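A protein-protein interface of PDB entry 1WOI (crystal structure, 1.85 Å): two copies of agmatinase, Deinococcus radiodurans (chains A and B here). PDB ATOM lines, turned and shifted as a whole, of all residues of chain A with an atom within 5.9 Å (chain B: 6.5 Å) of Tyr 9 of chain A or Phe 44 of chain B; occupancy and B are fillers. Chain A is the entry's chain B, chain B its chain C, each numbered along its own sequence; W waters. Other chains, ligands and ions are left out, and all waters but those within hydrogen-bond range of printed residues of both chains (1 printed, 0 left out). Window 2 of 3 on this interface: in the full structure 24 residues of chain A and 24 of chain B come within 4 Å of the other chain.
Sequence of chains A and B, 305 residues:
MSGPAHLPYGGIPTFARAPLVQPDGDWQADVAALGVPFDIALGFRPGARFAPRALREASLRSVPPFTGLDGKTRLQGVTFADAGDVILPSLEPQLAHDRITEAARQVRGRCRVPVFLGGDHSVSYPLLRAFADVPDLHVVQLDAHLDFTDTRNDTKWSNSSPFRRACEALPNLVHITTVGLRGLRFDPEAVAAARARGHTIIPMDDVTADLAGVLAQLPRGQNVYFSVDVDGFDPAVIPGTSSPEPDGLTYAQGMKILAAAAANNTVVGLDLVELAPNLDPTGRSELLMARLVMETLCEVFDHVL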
ATOM      1  N   LEU A   7     -17.618  -4.799 -12.569  1.00  0.00           N
ATOM      2  CA  LEU A   7     -17.733  -3.353 -12.688  1.00  0.00           C
ATOM      3  C   LEU A   7     -16.858  -3.048 -13.903  1.00  0.00           C
ATOM      4  O   LEU A   7     -16.082  -3.903 -14.330  1.00  0.00           O
ATOM      5  CB  LEU A   7     -17.181  -2.652 -11.444  1.00  0.00           C
ATOM      6  CG  LEU A   7     -18.069  -2.554 -10.197  1.00  0.00           C
ATOM      7  CD1 LEU A   7     -19.343  -1.805 -10.550  1.00  0.00           C
ATOM      8  CD2 LEU A   7     -18.387  -3.941  -9.660  1.00  0.00           C
ATOM      9  N   PRO A   8     -16.967  -1.837 -14.474  1.00  0.00           N
ATOM     10  CA  PRO A   8     -16.170  -1.460 -15.647  1.00  0.00           C
ATOM     11  C   PRO A   8     -14.666  -1.722 -15.559  1.00  0.00           C
ATOM     12  O   PRO A   8     -14.033  -2.037 -16.568  1.00  0.00           O
ATOM     13  CB  PRO A   8     -16.495   0.022 -15.813  1.00  0.00           C
ATOM     14  CG  PRO A   8     -17.920   0.083 -15.382  1.00  0.00           C
ATOM     15  CD  PRO A   8     -17.910  -0.760 -14.121  1.00  0.00           C
ATOM     16  N   TYR A   9     -14.094  -1.597 -14.363  1.00  0.00           N
ATOM     17  CA  TYR A   9     -12.660  -1.816 -14.187  1.00  0.00           C
ATOM     18  C   TYR A   9     -12.273  -3.273 -13.958  1.00  0.00           C
ATOM     19  O   TYR A   9     -11.086  -3.598 -13.880  1.00  0.00           O
ATOM     20  CB  TYR A   9     -12.122  -0.976 -13.023  1.00  0.00           C
ATOM     21  CG  TYR A   9     -12.953  -1.037 -11.759  1.00  0.00           C
ATOM     22  CD1 TYR A   9     -13.900  -0.052 -11.483  1.00  0.00           C
ATOM     23  CD2 TYR A   9     -12.794  -2.073 -10.838  1.00  0.00           C
ATOM     24  CE1 TYR A   9     -14.668  -0.091 -10.323  1.00  0.00           C
ATOM     25  CE2 TYR A   9     -13.562  -2.123  -9.670  1.00  0.00           C
ATOM     26  CZ  TYR A   9     -14.498  -1.128  -9.421  1.00  0.00           C
ATOM     27  OH  TYR A   9     -15.275  -1.162  -8.279  1.00  0.00           O
ATOM     28  N   GLY A  10     -13.264  -4.150 -13.848  1.00  0.00           N
ATOM     29  CA  GLY A  10     -12.957  -5.548 -13.614  1.00  0.00           C
ATOM     30  C   GLY A  10     -13.121  -6.445 -14.825  1.00  0.00           C
ATOM     31  O   GLY A  10     -13.903  -6.152 -15.733  1.00  0.00           O
ATOM     32  N   GLY A  11     -12.367  -7.540 -14.835  1.00  0.00           N
ATOM     33  CA  GLY A  11     -12.452  -8.501 -15.916  1.00  0.00           C
ATOM     34  C   GLY A  11     -11.552  -8.246 -17.104  1.00  0.00           C
ATOM     35  O   GLY A  11     -10.978  -7.162 -17.254  1.00  0.00           O
ATOM     36  N   ARG A  17     -17.666  -7.076 -23.686  1.00  0.00           N
ATOM     37  CA  ARG A  17     -17.471  -8.167 -22.739  1.00  0.00           C
ATOM     38  C   ARG A  17     -17.985  -9.469 -23.355  1.00  0.00           C
ATOM     39  O   ARG A  17     -18.476 -10.358 -22.656  1.00  0.00           O
ATOM     40  CB  ARG A  17     -18.203  -7.860 -21.423  1.00  0.00           C
ATOM     41  CG  ARG A  17     -17.544  -8.465 -20.181  1.00  0.00           C
ATOM     42  CD  ARG A  17     -18.356  -8.203 -18.910  1.00  0.00           C
ATOM     43  NE  ARG A  17     -18.089  -6.916 -18.261  1.00  0.00           N
ATOM     44  CZ  ARG A  17     -16.943  -6.588 -17.662  1.00  0.00           C
ATOM     45  NH1 ARG A  17     -15.933  -7.447 -17.632  1.00  0.00           N
ATOM     46  NH2 ARG A  17     -16.818  -5.411 -17.058  1.00  0.00           N
ATOM     47  N   GLU A  57     -11.758  -1.744 -23.627  1.00  0.00           N
ATOM     48  CA  GLU A  57     -11.884  -1.347 -22.232  1.00  0.00           C
ATOM     49  C   GLU A  57     -13.067  -0.401 -22.032  1.00  0.00           C
ATOM     50  O   GLU A  57     -13.860  -0.569 -21.104  1.00  0.00           O
ATOM     51  CB  GLU A  57     -10.590  -0.673 -21.770  1.00  0.00           C
ATOM     52  CG  GLU A  57      -9.403  -1.616 -21.740  1.00  0.00           C
ATOM     53  CD  GLU A  57      -8.076  -0.895 -21.611  1.00  0.00           C
ATOM     54  OE1 GLU A  57      -7.041  -1.585 -21.515  1.00  0.00           O
ATOM     55  OE2 GLU A  57      -8.063   0.355 -21.609  1.00  0.00           O
ATOM     56  N   LEU A  60     -16.750  -1.708 -21.857  1.00  0.00           N
ATOM     57  CA  LEU A  60     -17.240  -2.343 -20.641  1.00  0.00           C
ATOM     58  C   LEU A  60     -18.235  -1.417 -19.953  1.00  0.00           C
ATOM     59  O   LEU A  60     -18.974  -1.831 -19.061  1.00  0.00           O
ATOM     60  CB  LEU A  60     -16.069  -2.692 -19.716  1.00  0.00           C
ATOM     61  CG  LEU A  60     -15.073  -3.669 -20.349  1.00  0.00           C
ATOM     62  CD1 LEU A  60     -14.027  -4.084 -19.322  1.00  0.00           C
ATOM     63  CD2 LEU A  60     -15.820  -4.900 -20.871  1.00  0.00           C
ATOM     64  N   ARG A  61     -18.246  -0.158 -20.377  1.00  0.00           N
ATOM     65  CA  ARG A  61     -19.177   0.828 -19.842  1.00  0.00           C
ATOM     66  C   ARG A  61     -20.485   0.705 -20.621  1.00  0.00           C
ATOM     67  O   ARG A  61     -21.521   1.212 -20.193  1.00  0.00           O
ATOM     68  CB  ARG A  61     -18.624   2.244 -20.026  1.00  0.00           C
ATOM     69  CG  ARG A  61     -17.489   2.611 -19.092  1.00  0.00           C
ATOM     70  CD  ARG A  61     -17.994   3.431 -17.925  1.00  0.00           C
ATOM     71  NE  ARG A  61     -19.121   2.795 -17.253  1.00  0.00           N
ATOM     72  CZ  ARG A  61     -19.667   3.243 -16.127  1.00  0.00           C
ATOM     73  NH1 ARG A  61     -19.187   4.331 -15.544  1.00  0.00           N
ATOM     74  NH2 ARG A  61     -20.693   2.602 -15.584  1.00  0.00           N
ATOM     75  N   LEU A 287     -14.294   6.398 -24.445  1.00  0.00           N
ATOM     76  CA  LEU A 287     -15.594   6.128 -23.830  1.00  0.00           C
ATOM     77  C   LEU A 287     -16.749   6.500 -24.761  1.00  0.00           C
ATOM     78  O   LEU A 287     -17.694   5.727 -24.939  1.00  0.00           O
ATOM     79  CB  LEU A 287     -15.736   6.892 -22.508  1.00  0.00           C
ATOM     80  CG  LEU A 287     -14.897   6.378 -21.333  1.00  0.00           C
ATOM     81  CD1 LEU A 287     -15.123   7.254 -20.108  1.00  0.00           C
ATOM     82  CD2 LEU A 287     -15.286   4.939 -21.022  1.00  0.00           C
ATOM     83  N   LEU B  42     -18.344   4.953  -5.891  1.00  0.00           N
ATOM     84  CA  LEU B  42     -18.525   4.960  -7.340  1.00  0.00           C
ATOM     85  C   LEU B  42     -18.083   3.652  -7.987  1.00  0.00           C
ATOM     86  O   LEU B  42     -17.236   2.931  -7.455  1.00  0.00           O
ATOM     87  CB  LEU B  42     -17.826   6.179  -7.969  1.00  0.00           C
ATOM     88  CG  LEU B  42     -16.358   6.516  -7.728  1.00  0.00           C
ATOM     89  CD1 LEU B  42     -15.473   5.624  -8.601  1.00  0.00           C
ATOM     90  CD2 LEU B  42     -16.128   7.993  -8.085  1.00  0.00           C
ATOM     91  N   GLY B  43     -18.671   3.337  -9.134  1.00  0.00           N
ATOM     92  CA  GLY B  43     -18.343   2.081  -9.783  1.00  0.00           C
ATOM     93  C   GLY B  43     -17.322   2.087 -10.902  1.00  0.00           C
ATOM     94  O   GLY B  43     -17.094   1.047 -11.526  1.00  0.00           O
ATOM     95  N   PHE B  44     -16.688   3.225 -11.156  1.00  0.00           N
ATOM     96  CA  PHE B  44     -15.721   3.270 -12.240  1.00  0.00           C
ATOM     97  C   PHE B  44     -14.370   3.903 -11.890  1.00  0.00           C
ATOM     98  O   PHE B  44     -13.497   3.244 -11.331  1.00  0.00           O
ATOM     99  CB  PHE B  44     -16.341   3.992 -13.444  1.00  0.00           C
ATOM    100  CG  PHE B  44     -15.537   3.875 -14.708  1.00  0.00           C
ATOM    101  CD1 PHE B  44     -15.683   4.818 -15.722  1.00  0.00           C
ATOM    102  CD2 PHE B  44     -14.649   2.823 -14.895  1.00  0.00           C
ATOM    103  CE1 PHE B  44     -14.950   4.712 -16.905  1.00  0.00           C
ATOM    104  CE2 PHE B  44     -13.916   2.707 -16.072  1.00  0.00           C
ATOM    105  CZ  PHE B  44     -14.070   3.658 -17.079  1.00  0.00           C
ATOM    106  N   ARG B  45     -14.206   5.180 -12.223  1.00  0.00           N
ATOM    107  CA  ARG B  45     -12.948   5.886 -11.987  1.00  0.00           C
ATOM    108  C   ARG B  45     -12.924   6.797 -10.757  1.00  0.00           C
ATOM    109  O   ARG B  45     -13.627   7.803 -10.701  1.00  0.00           O
ATOM    110  CB  ARG B  45     -12.589   6.697 -13.237  1.00  0.00           C
ATOM    111  CG  ARG B  45     -12.440   5.844 -14.492  1.00  0.00           C
ATOM    112  CD  ARG B  45     -12.005   6.682 -15.680  1.00  0.00           C
ATOM    113  NE  ARG B  45     -12.998   7.691 -16.030  1.00  0.00           N
ATOM    114  CZ  ARG B  45     -12.827   8.602 -16.984  1.00  0.00           C
ATOM    115  NH1 ARG B  45     -11.699   8.624 -17.681  1.00  0.00           N
ATOM    116  NH2 ARG B  45     -13.781   9.488 -17.239  1.00  0.00           N
ATOM    117  N   PRO B  46     -12.088   6.461  -9.761  1.00  0.00           N
ATOM    118  CA  PRO B  46     -11.931   7.214  -8.507  1.00  0.00           C
ATOM    119  C   PRO B  46     -11.266   8.571  -8.731  1.00  0.00           C
ATOM    120  O   PRO B  46     -10.661   8.806  -9.775  1.00  0.00           O
ATOM    121  CB  PRO B  46     -11.025   6.313  -7.661  1.00  0.00           C
ATOM    122  CG  PRO B  46     -11.137   4.971  -8.296  1.00  0.00           C
ATOM    123  CD  PRO B  46     -11.222   5.274  -9.759  1.00  0.00           C
ATOM    124  N   ARG B 152     -27.334  -2.056  -6.403  1.00  0.00           N
ATOM    125  CA  ARG B 152     -26.396  -2.138  -7.514  1.00  0.00           C
ATOM    126  C   ARG B 152     -25.120  -2.808  -7.007  1.00  0.00           C
ATOM    127  O   ARG B 152     -24.620  -2.472  -5.934  1.00  0.00           O
ATOM    128  CB  ARG B 152     -26.064  -0.734  -8.033  1.00  0.00           C
ATOM    129  CG  ARG B 152     -25.384  -0.711  -9.390  1.00  0.00           C
ATOM    130  CD  ARG B 152     -24.538   0.542  -9.556  1.00  0.00           C
ATOM    131  NE  ARG B 152     -23.299   0.446  -8.785  1.00  0.00           N
ATOM    132  CZ  ARG B 152     -22.417   1.430  -8.655  1.00  0.00           C
ATOM    133  NH1 ARG B 152     -21.318   1.243  -7.934  1.00  0.00           N
ATOM    134  NH2 ARG B 152     -22.637   2.602  -9.237  1.00  0.00           N
ATOM    135  N   THR B 241     -14.618  13.746 -14.739  1.00  0.00           N
ATOM    136  CA  THR B 241     -15.650  13.021 -14.007  1.00  0.00           C
ATOM    137  C   THR B 241     -15.580  11.535 -14.364  1.00  0.00           C
ATOM    138  O   THR B 241     -15.160  11.160 -15.463  1.00  0.00           O
ATOM    139  CB  THR B 241     -17.053  13.609 -14.298  1.00  0.00           C
ATOM    140  OG1 THR B 241     -17.982  13.134 -13.316  1.00  0.00           O
ATOM    141  CG2 THR B 241     -17.541  13.201 -15.676  1.00  0.00           C
ATOM    142  N   SER B 242     -15.986  10.685 -13.429  1.00  0.00           N
ATOM    143  CA  SER B 242     -15.916   9.241 -13.626  1.00  0.00           C
ATOM    144  C   SER B 242     -16.623   8.655 -14.845  1.00  0.00           C
ATOM    145  O   SER B 242     -16.018   7.916 -15.627  1.00  0.00           O
ATOM    146  CB  SER B 242     -16.439   8.521 -12.377  1.00  0.00           C
ATOM    147  OG  SER B 242     -16.395   7.109 -12.555  1.00  0.00           O
ATOM    148  N   SER B 243     -17.901   8.975 -14.999  1.00  0.00           N
ATOM    149  CA  SER B 243     -18.693   8.404 -16.080  1.00  0.00           C
ATOM    150  C   SER B 243     -19.366   9.439 -16.957  1.00  0.00           C
ATOM    151  O   SER B 243     -20.550   9.726 -16.794  1.00  0.00           O
ATOM    152  CB  SER B 243     -19.758   7.485 -15.482  1.00  0.00           C
ATOM    153  OG  SER B 243     -19.187   6.633 -14.507  1.00  0.00           O
ATOM    154  N   PRO B 244     -18.619  10.009 -17.908  1.00  0.00           N
ATOM    155  CA  PRO B 244     -19.180  11.021 -18.803  1.00  0.00           C
ATOM    156  C   PRO B 244     -20.119  10.439 -19.848  1.00  0.00           C
ATOM    157  O   PRO B 244     -19.975   9.283 -20.271  1.00  0.00           O
ATOM    158  CB  PRO B 244     -17.937  11.661 -19.420  1.00  0.00           C
ATOM    159  CG  PRO B 244     -16.982  10.509 -19.491  1.00  0.00           C
ATOM    160  CD  PRO B 244     -17.176   9.830 -18.149  1.00  0.00           C
HETATM  161  O   HOH W   1     -17.340   0.182  -6.805  1.00  0.00           O
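OG of Ser 243 of chain B lies within hydrogen-bond range of NH1 of Arg 61 of chain A (2.5 Å).
The backbone carbonyl oxygen of Leu 7 of chain A sits at hydrogen-bond distance from the guanidinium group of Arg 17 of chain A, 3.2 Å away.
The backbone NH of Arg 45 of chain B is in hydrogen-bond range of the side-chain hydroxyl of Ser 242 of chain B, at 2.9 Å.
The guanidinium group (NH2) of Arg 45 of chain B sits at hydrogen-bond distance from the backbone carbonyl oxygen (O) of Thr 241 of chain B (2.8 Å).
OG of Ser 243 of chain B lies close to OG of Ser 242 of chain B, 3.4 Å away.
Among the printed residues, merely in contact across the chains: Leu 7 of chain A with Gly 43 of chain B, Pro 8 of chain A with Gly 43 of chain B, Pro 8 of chain A with Phe 44 of chain B, Tyr 9 of chain A with Gly 43 of chain B, Tyr 9 of chain A with Phe 44 of chain B, Arg 61 of chain A with Phe 44 of chain B, Leu 287 of chain A with Arg 45 of chain B and Leu 287 of chain A with Pro 244 of chain B.
Tyr 9 of chain A touches just these residues of chain B: Gly 43 and Phe 44.
Printed residues of chain B within 4 Å of Leu 7 of chain A: Gly 43.
Printed residues of chain B within 4 Å of Arg 61 of chain A: Phe 44 and Ser 243.
Of the printed residues of chain A, Gly 43 of chain B touches Leu 7 (3.7 Å), Pro 8 (3.3 Å) and Tyr 9 (2.9 Å).
Of the printed residues of chain A, Ser 243 of chain B touches Arg 61 (2.5 Å).
Gly 10 of chain A touches none of the printed residues of chain B.
Thr 241 of chain B touches none of the printed residues of chain A.
The nearest residue of chain A that does not touch Phe 44 of chain B is Leu 287 of chain A (4.1 Å).
The nearest printed residue of chain A that does not touch Pro 244 of chain B is Arg 61 of chain A (6.2 Å).
Hydrophobic or aromatic side chains of chain A that line the printed part of chain B: Leu 7, Pro 8, Tyr 9 and Leu 287.
Along chain B the printed residues that touch a printed residue of chain A span positions 43 to 244.
No position is printed for both chains.
Of the 9 pairs that touch across the chains among the printed residues, none has its exchanged pair printed and touching as well.
Water W1 bridges the backbone carbonyl oxygen of Leu 42 of chain B and the side-chain hydroxyl of Tyr 9 of chain A.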
